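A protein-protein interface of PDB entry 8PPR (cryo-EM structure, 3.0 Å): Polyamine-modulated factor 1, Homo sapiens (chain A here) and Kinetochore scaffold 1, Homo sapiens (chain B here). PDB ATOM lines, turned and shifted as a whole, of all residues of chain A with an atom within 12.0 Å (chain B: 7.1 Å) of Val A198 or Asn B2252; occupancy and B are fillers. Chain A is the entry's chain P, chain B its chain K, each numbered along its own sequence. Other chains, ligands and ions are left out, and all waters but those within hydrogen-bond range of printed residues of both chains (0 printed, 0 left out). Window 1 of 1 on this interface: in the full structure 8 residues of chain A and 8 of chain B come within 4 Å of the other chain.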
ATOM      1  N   LEU A 190     -27.239   8.279 -16.304  1.00  0.00           N
ATOM      2  CA  LEU A 190     -26.129   8.680 -17.160  1.00  0.00           C
ATOM      3  C   LEU A 190     -25.485   7.503 -17.880  1.00  0.00           C
ATOM      4  O   LEU A 190     -24.672   7.720 -18.788  1.00  0.00           O
ATOM      5  CB  LEU A 190     -25.071   9.404 -16.328  1.00  0.00           C
ATOM      6  CG  LEU A 190     -25.558  10.512 -15.393  1.00  0.00           C
ATOM      7  CD1 LEU A 190     -24.389  11.163 -14.672  1.00  0.00           C
ATOM      8  CD2 LEU A 190     -26.356  11.550 -16.160  1.00  0.00           C
ATOM      9  N   HIS A 191     -25.822   6.271 -17.488  1.00  0.00           N
ATOM     10  CA  HIS A 191     -25.155   5.095 -18.035  1.00  0.00           C
ATOM     11  C   HIS A 191     -25.405   4.949 -19.528  1.00  0.00           C
ATOM     12  O   HIS A 191     -24.498   4.576 -20.280  1.00  0.00           O
ATOM     13  CB  HIS A 191     -25.619   3.845 -17.292  1.00  0.00           C
ATOM     14  CG  HIS A 191     -25.199   2.564 -17.941  1.00  0.00           C
ATOM     15  ND1 HIS A 191     -24.011   1.932 -17.643  1.00  0.00           N
ATOM     16  CD2 HIS A 191     -25.816   1.788 -18.864  1.00  0.00           C
ATOM     17  CE1 HIS A 191     -23.911   0.827 -18.358  1.00  0.00           C
ATOM     18  NE2 HIS A 191     -24.992   0.716 -19.109  1.00  0.00           N
ATOM     19  N   ARG A 192     -26.636   5.205 -19.975  1.00  0.00           N
ATOM     20  CA  ARG A 192     -26.939   5.055 -21.394  1.00  0.00           C
ATOM     21  C   ARG A 192     -26.113   6.018 -22.234  1.00  0.00           C
ATOM     22  O   ARG A 192     -25.539   5.628 -23.258  1.00  0.00           O
ATOM     23  CB  ARG A 192     -28.430   5.272 -21.641  1.00  0.00           C
ATOM     24  CG  ARG A 192     -28.848   5.027 -23.077  1.00  0.00           C
ATOM     25  CD  ARG A 192     -30.185   5.671 -23.383  1.00  0.00           C
ATOM     26  NE  ARG A 192     -31.300   4.895 -22.855  1.00  0.00           N
ATOM     27  CZ  ARG A 192     -32.012   4.031 -23.565  1.00  0.00           C
ATOM     28  NH1 ARG A 192     -31.728   3.778 -24.832  1.00  0.00           N
ATOM     29  NH2 ARG A 192     -33.032   3.401 -22.988  1.00  0.00           N
ATOM     30  N   GLU A 193     -26.029   7.279 -21.807  1.00  0.00           N
ATOM     31  CA  GLU A 193     -25.216   8.250 -22.529  1.00  0.00           C
ATOM     32  C   GLU A 193     -23.743   7.874 -22.490  1.00  0.00           C
ATOM     33  O   GLU A 193     -23.028   8.035 -23.487  1.00  0.00           O
ATOM     34  CB  GLU A 193     -25.429   9.648 -21.949  1.00  0.00           C
ATOM     35  CG  GLU A 193     -26.834   9.904 -21.428  1.00  0.00           C
ATOM     36  CD  GLU A 193     -27.874  10.019 -22.531  1.00  0.00           C
ATOM     37  OE1 GLU A 193     -27.513   9.910 -23.723  1.00  0.00           O
ATOM     38  OE2 GLU A 193     -29.061  10.218 -22.202  1.00  0.00           O
ATOM     39  N   GLN A 194     -23.265   7.381 -21.346  1.00  0.00           N
ATOM     40  CA  GLN A 194     -21.862   6.993 -21.251  1.00  0.00           C
ATOM     41  C   GLN A 194     -21.538   5.844 -22.197  1.00  0.00           C
ATOM     42  O   GLN A 194     -20.511   5.866 -22.886  1.00  0.00           O
ATOM     43  CB  GLN A 194     -21.523   6.619 -19.811  1.00  0.00           C
ATOM     44  CG  GLN A 194     -21.239   7.813 -18.923  1.00  0.00           C
ATOM     45  CD  GLN A 194     -21.356   7.480 -17.453  1.00  0.00           C
ATOM     46  OE1 GLN A 194     -21.947   6.468 -17.079  1.00  0.00           O
ATOM     47  NE2 GLN A 194     -20.782   8.327 -16.609  1.00  0.00           N
ATOM     48  N   ARG A 195     -22.411   4.837 -22.257  1.00  0.00           N
ATOM     49  CA  ARG A 195     -22.176   3.725 -23.168  1.00  0.00           C
ATOM     50  C   ARG A 195     -22.301   4.162 -24.619  1.00  0.00           C
ATOM     51  O   ARG A 195     -21.563   3.669 -25.479  1.00  0.00           O
ATOM     52  CB  ARG A 195     -23.142   2.580 -22.868  1.00  0.00           C
ATOM     53  CG  ARG A 195     -23.031   2.046 -21.452  1.00  0.00           C
ATOM     54  CD  ARG A 195     -21.605   1.641 -21.116  1.00  0.00           C
ATOM     55  NE  ARG A 195     -21.113   0.573 -21.978  1.00  0.00           N
ATOM     56  CZ  ARG A 195     -19.838   0.222 -22.079  1.00  0.00           C
ATOM     57  NH1 ARG A 195     -18.894   0.840 -21.389  1.00  0.00           N
ATOM     58  NH2 ARG A 195     -19.502  -0.775 -22.892  1.00  0.00           N
ATOM     59  N   GLU A 196     -23.213   5.091 -24.911  1.00  0.00           N
ATOM     60  CA  GLU A 196     -23.301   5.629 -26.263  1.00  0.00           C
ATOM     61  C   GLU A 196     -22.015   6.347 -26.649  1.00  0.00           C
ATOM     62  O   GLU A 196     -21.526   6.202 -27.775  1.00  0.00           O
ATOM     63  CB  GLU A 196     -24.496   6.573 -26.374  1.00  0.00           C
ATOM     64  CG  GLU A 196     -24.679   7.165 -27.757  1.00  0.00           C
ATOM     65  CD  GLU A 196     -24.929   6.108 -28.814  1.00  0.00           C
ATOM     66  OE1 GLU A 196     -25.506   5.051 -28.481  1.00  0.00           O
ATOM     67  OE2 GLU A 196     -24.543   6.333 -29.980  1.00  0.00           O
ATOM     68  N   LEU A 197     -21.455   7.127 -25.725  1.00  0.00           N
ATOM     69  CA  LEU A 197     -20.189   7.799 -25.990  1.00  0.00           C
ATOM     70  C   LEU A 197     -19.073   6.790 -26.216  1.00  0.00           C
ATOM     71  O   LEU A 197     -18.236   6.965 -27.110  1.00  0.00           O
ATOM     72  CB  LEU A 197     -19.840   8.734 -24.835  1.00  0.00           C
ATOM     73  CG  LEU A 197     -18.566   9.558 -25.008  1.00  0.00           C
ATOM     74  CD1 LEU A 197     -18.542  10.218 -26.377  1.00  0.00           C
ATOM     75  CD2 LEU A 197     -18.455  10.598 -23.906  1.00  0.00           C
ATOM     76  N   VAL A 198     -19.042   5.730 -25.408  1.00  0.00           N
ATOM     77  CA  VAL A 198     -18.044   4.680 -25.596  1.00  0.00           C
ATOM     78  C   VAL A 198     -18.190   4.058 -26.978  1.00  0.00           C
ATOM     79  O   VAL A 198     -17.197   3.768 -27.655  1.00  0.00           O
ATOM     80  CB  VAL A 198     -18.162   3.627 -24.481  1.00  0.00           C
ATOM     81  CG1 VAL A 198     -17.316   2.407 -24.805  1.00  0.00           C
ATOM     82  CG2 VAL A 198     -17.749   4.223 -23.146  1.00  0.00           C
ATOM     83  N   ALA A 199     -19.431   3.851 -27.418  1.00  0.00           N
ATOM     84  CA  ALA A 199     -19.663   3.330 -28.760  1.00  0.00           C
ATOM     85  C   ALA A 199     -19.157   4.300 -29.820  1.00  0.00           C
ATOM     86  O   ALA A 199     -18.574   3.883 -30.828  1.00  0.00           O
ATOM     87  CB  ALA A 199     -21.150   3.042 -28.962  1.00  0.00           C
ATOM     88  N   VAL A 200     -19.373   5.599 -29.610  1.00  0.00           N
ATOM     89  CA  VAL A 200     -18.890   6.597 -30.558  1.00  0.00           C
ATOM     90  C   VAL A 200     -17.369   6.577 -30.619  1.00  0.00           C
ATOM     91  O   VAL A 200     -16.773   6.565 -31.702  1.00  0.00           O
ATOM     92  CB  VAL A 200     -19.419   7.992 -30.182  1.00  0.00           C
ATOM     93  CG1 VAL A 200     -18.736   9.062 -31.019  1.00  0.00           C
ATOM     94  CG2 VAL A 200     -20.925   8.053 -30.359  1.00  0.00           C
ATOM     95  N   LEU A 201     -16.720   6.560 -29.457  1.00  0.00           N
ATOM     96  CA  LEU A 201     -15.262   6.523 -29.379  1.00  0.00           C
ATOM     97  C   LEU A 201     -14.843   5.071 -29.178  1.00  0.00           C
ATOM     98  O   LEU A 201     -14.529   4.625 -28.075  1.00  0.00           O
ATOM     99  CB  LEU A 201     -14.761   7.423 -28.256  1.00  0.00           C
ATOM    100  CG  LEU A 201     -15.431   8.795 -28.177  1.00  0.00           C
ATOM    101  CD1 LEU A 201     -14.913   9.575 -26.981  1.00  0.00           C
ATOM    102  CD2 LEU A 201     -15.215   9.571 -29.466  1.00  0.00           C
ATOM    103  N   ARG A 202     -14.840   4.329 -30.277  1.00  0.00           N
ATOM    104  CA  ARG A 202     -14.554   2.906 -30.253  1.00  0.00           C
ATOM    105  C   ARG A 202     -13.070   2.649 -30.478  1.00  0.00           C
ATOM    106  O   ARG A 202     -12.345   3.472 -31.041  1.00  0.00           O
ATOM    107  CB  ARG A 202     -15.378   2.179 -31.315  1.00  0.00           C
ATOM    108  CG  ARG A 202     -14.912   2.460 -32.725  1.00  0.00           C
ATOM    109  CD  ARG A 202     -16.020   2.198 -33.722  1.00  0.00           C
ATOM    110  NE  ARG A 202     -16.835   3.390 -33.924  1.00  0.00           N
ATOM    111  CZ  ARG A 202     -16.445   4.465 -34.596  1.00  0.00           C
ATOM    112  NH1 ARG A 202     -15.252   4.531 -35.165  1.00  0.00           N
ATOM    113  NH2 ARG A 202     -17.273   5.501 -34.699  1.00  0.00           N
ATOM    114  N   GLU A 203     -12.629   1.481 -30.021  1.00  0.00           N
ATOM    115  CA  GLU A 203     -11.249   1.077 -30.185  1.00  0.00           C
ATOM    116  C   GLU A 203     -10.963   0.763 -31.651  1.00  0.00           C
ATOM    117  O   GLU A 203     -11.877   0.442 -32.416  1.00  0.00           O
ATOM    118  CB  GLU A 203     -10.960  -0.138 -29.307  1.00  0.00           C
ATOM    119  CG  GLU A 203     -11.480   0.011 -27.885  1.00  0.00           C
ATOM    120  CD  GLU A 203     -11.062  -1.131 -26.982  1.00  0.00           C
ATOM    121  OE1 GLU A 203     -10.204  -1.935 -27.396  1.00  0.00           O
ATOM    122  OE2 GLU A 203     -11.589  -1.219 -25.853  1.00  0.00           O
ATOM    123  N   PRO A 204      -9.695   0.871 -32.076  1.00  0.00           N
ATOM    124  CA  PRO A 204      -9.304   0.556 -33.454  1.00  0.00           C
ATOM    125  C   PRO A 204      -9.660  -0.872 -33.855  1.00  0.00           C
ATOM    126  O   PRO A 204      -9.555  -1.765 -33.014  1.00  0.00           O
ATOM    127  CB  PRO A 204      -7.787   0.747 -33.439  1.00  0.00           C
ATOM    128  CG  PRO A 204      -7.548   1.730 -32.356  1.00  0.00           C
ATOM    129  CD  PRO A 204      -8.573   1.431 -31.303  1.00  0.00           C
ATOM    130  N   ARG B2248      -5.034   3.007 -22.521  1.00  0.00           N
ATOM    131  CA  ARG B2248      -5.767   3.859 -23.447  1.00  0.00           C
ATOM    132  C   ARG B2248      -7.246   3.502 -23.527  1.00  0.00           C
ATOM    133  O   ARG B2248      -8.103   4.386 -23.431  1.00  0.00           O
ATOM    134  CB  ARG B2248      -5.143   3.780 -24.843  1.00  0.00           C
ATOM    135  CG  ARG B2248      -5.928   4.546 -25.886  1.00  0.00           C
ATOM    136  CD  ARG B2248      -5.898   6.033 -25.586  1.00  0.00           C
ATOM    137  NE  ARG B2248      -6.629   6.808 -26.579  1.00  0.00           N
ATOM    138  CZ  ARG B2248      -7.921   7.098 -26.495  1.00  0.00           C
ATOM    139  NH1 ARG B2248      -8.655   6.692 -25.472  1.00  0.00           N
ATOM    140  NH2 ARG B2248      -8.489   7.812 -27.462  1.00  0.00           N
ATOM    141  N   TRP B2249      -7.565   2.220 -23.701  1.00  0.00           N
ATOM    142  CA  TRP B2249      -8.934   1.775 -23.928  1.00  0.00           C
ATOM    143  C   TRP B2249      -9.515   1.020 -22.740  1.00  0.00           C
ATOM    144  O   TRP B2249     -10.478   0.264 -22.902  1.00  0.00           O
ATOM    145  CB  TRP B2249      -8.993   0.916 -25.190  1.00  0.00           C
ATOM    146  CG  TRP B2249      -8.432   1.610 -26.385  1.00  0.00           C
ATOM    147  CD1 TRP B2249      -7.263   1.326 -27.022  1.00  0.00           C
ATOM    148  CD2 TRP B2249      -9.024   2.701 -27.097  1.00  0.00           C
ATOM    149  NE1 TRP B2249      -7.084   2.179 -28.085  1.00  0.00           N
ATOM    150  CE2 TRP B2249      -8.154   3.032 -28.153  1.00  0.00           C
ATOM    151  CE3 TRP B2249     -10.205   3.431 -26.941  1.00  0.00           C
ATOM    152  CZ2 TRP B2249      -8.427   4.062 -29.048  1.00  0.00           C
ATOM    153  CZ3 TRP B2249     -10.475   4.452 -27.833  1.00  0.00           C
ATOM    154  CH2 TRP B2249      -9.589   4.758 -28.872  1.00  0.00           C
ATOM    155  N   GLY B2250      -8.952   1.208 -21.551  1.00  0.00           N
ATOM    156  CA  GLY B2250      -9.424   0.534 -20.364  1.00  0.00           C
ATOM    157  C   GLY B2250     -10.865   0.826 -19.989  1.00  0.00           C
ATOM    158  O   GLY B2250     -11.646  -0.092 -19.723  1.00  0.00           O
ATOM    159  N   PRO B2251     -11.251   2.106 -19.946  1.00  0.00           N
ATOM    160  CA  PRO B2251     -12.638   2.431 -19.578  1.00  0.00           C
ATOM    161  C   PRO B2251     -13.675   1.859 -20.524  1.00  0.00           C
ATOM    162  O   PRO B2251     -14.826   1.671 -20.111  1.00  0.00           O
ATOM    163  CB  PRO B2251     -12.650   3.963 -19.593  1.00  0.00           C
ATOM    164  CG  PRO B2251     -11.260   4.329 -19.241  1.00  0.00           C
ATOM    165  CD  PRO B2251     -10.402   3.313 -19.945  1.00  0.00           C
ATOM    166  N   ASN B2252     -13.315   1.582 -21.779  1.00  0.00           N
ATOM    167  CA  ASN B2252     -14.245   0.897 -22.670  1.00  0.00           C
ATOM    168  C   ASN B2252     -14.589  -0.489 -22.144  1.00  0.00           C
ATOM    169  O   ASN B2252     -15.687  -0.996 -22.396  1.00  0.00           O
ATOM    170  CB  ASN B2252     -13.657   0.802 -24.077  1.00  0.00           C
ATOM    171  CG  ASN B2252     -13.803   2.093 -24.858  1.00  0.00           C
ATOM    172  OD1 ASN B2252     -13.992   3.164 -24.281  1.00  0.00           O
ATOM    173  ND2 ASN B2252     -13.718   1.998 -26.181  1.00  0.00           N
ATOM    174  N   TYR B2253     -13.668  -1.110 -21.412  1.00  0.00           N
ATOM    175  CA  TYR B2253     -13.879  -2.420 -20.817  1.00  0.00           C
ATOM    176  C   TYR B2253     -14.118  -2.342 -19.316  1.00  0.00           C
ATOM    177  O   TYR B2253     -13.912  -3.336 -18.614  1.00  0.00           O
ATOM    178  CB  TYR B2253     -12.684  -3.323 -21.110  1.00  0.00           C
ATOM    179  CG  TYR B2253     -12.523  -3.637 -22.577  1.00  0.00           C
ATOM    180  CD1 TYR B2253     -13.620  -3.643 -23.426  1.00  0.00           C
ATOM    181  CD2 TYR B2253     -11.275  -3.919 -23.113  1.00  0.00           C
ATOM    182  CE1 TYR B2253     -13.480  -3.925 -24.769  1.00  0.00           C
ATOM    183  CE2 TYR B2253     -11.125  -4.203 -24.456  1.00  0.00           C
ATOM    184  CZ  TYR B2253     -12.230  -4.204 -25.278  1.00  0.00           C
ATOM    185  OH  TYR B2253     -12.086  -4.486 -26.617  1.00  0.00           O
ATOM    186  N   ASN B2254     -14.519  -1.174 -18.811  1.00  0.00           N
ATOM    187  CA  ASN B2254     -14.780  -0.902 -17.401  1.00  0.00           C
ATOM    188  C   ASN B2254     -13.523  -0.953 -16.546  1.00  0.00           C
ATOM    189  O   ASN B2254     -13.616  -0.875 -15.314  1.00  0.00           O
ATOM    190  CB  ASN B2254     -15.832  -1.852 -16.818  1.00  0.00           C
ATOM    191  CG  ASN B2254     -17.231  -1.509 -17.267  1.00  0.00           C
ATOM    192  OD1 ASN B2254     -17.814  -2.199 -18.103  1.00  0.00           O
ATOM    193  ND2 ASN B2254     -17.784  -0.437 -16.714  1.00  0.00           N
ATOM    194  N   LEU B2255     -12.350  -1.079 -17.158  1.00  0.00           N
ATOM    195  CA  LEU B2255     -11.088  -1.078 -16.425  1.00  0.00           C
ATOM    196  C   LEU B2255     -10.682   0.371 -16.196  1.00  0.00           C
ATOM    197  O   LEU B2255     -10.101   1.013 -17.072  1.00  0.00           O
ATOM    198  CB  LEU B2255     -10.020  -1.844 -17.196  1.00  0.00           C
ATOM    199  CG  LEU B2255      -8.594  -1.761 -16.661  1.00  0.00           C
ATOM    200  CD1 LEU B2255      -8.532  -2.234 -15.217  1.00  0.00           C
ATOM    201  CD2 LEU B2255      -7.672  -2.580 -17.541  1.00  0.00           C
ATOM    202  N   MET B2256     -10.993   0.895 -15.010  1.00  0.00           N
ATOM    203  CA  MET B2256     -10.765   2.310 -14.753  1.00  0.00           C
ATOM    204  C   MET B2256      -9.293   2.640 -14.565  1.00  0.00           C
ATOM    205  O   MET B2256      -8.829   3.672 -15.062  1.00  0.00           O
ATOM    206  CB  MET B2256     -11.538   2.756 -13.512  1.00  0.00           C
ATOM    207  CG  MET B2256     -13.045   2.694 -13.648  1.00  0.00           C
ATOM    208  SD  MET B2256     -13.697   3.760 -14.943  1.00  0.00           S
ATOM    209  CE  MET B2256     -14.013   2.563 -16.237  1.00  0.00           C
ATOM    210  N   TYR B2331     -15.008  -8.345 -19.079  1.00  0.00           N
ATOM    211  CA  TYR B2331     -16.068  -7.412 -19.438  1.00  0.00           C
ATOM    212  C   TYR B2331     -17.264  -8.147 -20.024  1.00  0.00           C
ATOM    213  O   TYR B2331     -18.416  -7.820 -19.719  1.00  0.00           O
ATOM    214  CB  TYR B2331     -15.544  -6.370 -20.423  1.00  0.00           C
ATOM    215  CG  TYR B2331     -16.643  -5.596 -21.111  1.00  0.00           C
ATOM    216  CD1 TYR B2331     -17.335  -4.597 -20.441  1.00  0.00           C
ATOM    217  CD2 TYR B2331     -16.992  -5.867 -22.426  1.00  0.00           C
ATOM    218  CE1 TYR B2331     -18.343  -3.888 -21.062  1.00  0.00           C
ATOM    219  CE2 TYR B2331     -18.000  -5.163 -23.056  1.00  0.00           C
ATOM    220  CZ  TYR B2331     -18.672  -4.175 -22.369  1.00  0.00           C
ATOM    221  OH  TYR B2331     -19.675  -3.469 -22.991  1.00  0.00           O
ATOM    222  N   HIS B2339     -24.710  -4.172 -18.736  1.00  0.00           N
ATOM    223  CA  HIS B2339     -24.783  -2.769 -19.129  1.00  0.00           C
ATOM    224  C   HIS B2339     -25.886  -2.490 -20.139  1.00  0.00           C
ATOM    225  O   HIS B2339     -26.195  -1.318 -20.385  1.00  0.00           O
ATOM    226  CB  HIS B2339     -23.437  -2.315 -19.693  1.00  0.00           C
ATOM    227  CG  HIS B2339     -22.360  -2.205 -18.660  1.00  0.00           C
ATOM    228  ND1 HIS B2339     -21.489  -1.139 -18.606  1.00  0.00           N
ATOM    229  CD2 HIS B2339     -22.031  -3.013 -17.626  1.00  0.00           C
ATOM    230  CE1 HIS B2339     -20.660  -1.302 -17.591  1.00  0.00           C
ATOM    231  NE2 HIS B2339     -20.968  -2.431 -16.979  1.00  0.00           N
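O of His B2339 lies within hydrogen-bond range of NE2 of His A191 (2.7 Å).
O of Leu A201 is in hydrogen-bond range of ND2 of Asn B2252 (3.3 Å).
NH2 of Arg A195 sits at hydrogen-bond distance from OH of Tyr B2331 (2.7 Å).
The side-chain carboxylate of Glu A203 sits close to the backbone carbonyl oxygen of Trp B2249 (3.5 Å).
OH of Tyr B2253 is in hydrogen-bond range of OE1 of Glu A203, 3.3 Å away.
The guanidinium group (NH2) of Arg A202 lies within hydrogen-bond range of the backbone carbonyl oxygen (O) of Val A200.
The side-chain amide oxygen (OD1) of Asn B2254 sits close to a ring nitrogen (NE2) of His B2339 (3.4 Å).
Among the printed residues, pairs that only touch across the chains: Glu A203 with Asn B2252, Val A198 with Asn B2252, Pro A204 with Trp B2249, Arg A202 with Trp B2249, Arg A195 with His B2339 and Arg A195 with Asn B2252.
Of chain B, only Asn B2252 (3.4 Å) comes within 4 Å of Val A198.
Asn B2252 touches four residues of chain A.
Trp B2249 touches three residues of chain A.
No residue of chain A comes within 4 Å of Pro B2251.
Of chain A, only Glu A203 (3.1 Å) comes within 4 Å of Tyr B2253.
Of the printed residues of chain B, Leu A201 touches Asn B2252.
Of the printed residues of chain B, Arg A202 touches Trp B2249.
Printed residues of chain B within 4 Å of Pro A204: Trp B2249.
Of the printed residues of chain B, Arg A195 touches Asn B2252 (3.8 Å), Tyr B2331 (2.7 Å) and His B2339 (3.7 Å).
Arg A192 touches none of the printed residues of chain B.
Glu A196 touches none of the printed residues of chain B.
The nearest residue of chain B that does not touch Val A198 is Pro B2251 (4.9 Å).
The nearest residue of chain A that does not touch Asn B2252 is Arg A202 (4.3 Å).
The nearest printed residue of chain B that does not touch Glu A203 is Gly B2250 (5.6 Å).
Of the 11 printed residues of chain B, 5 touch a printed residue of chain A.
Among the printed residues, 11 pairs touch across the chains.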
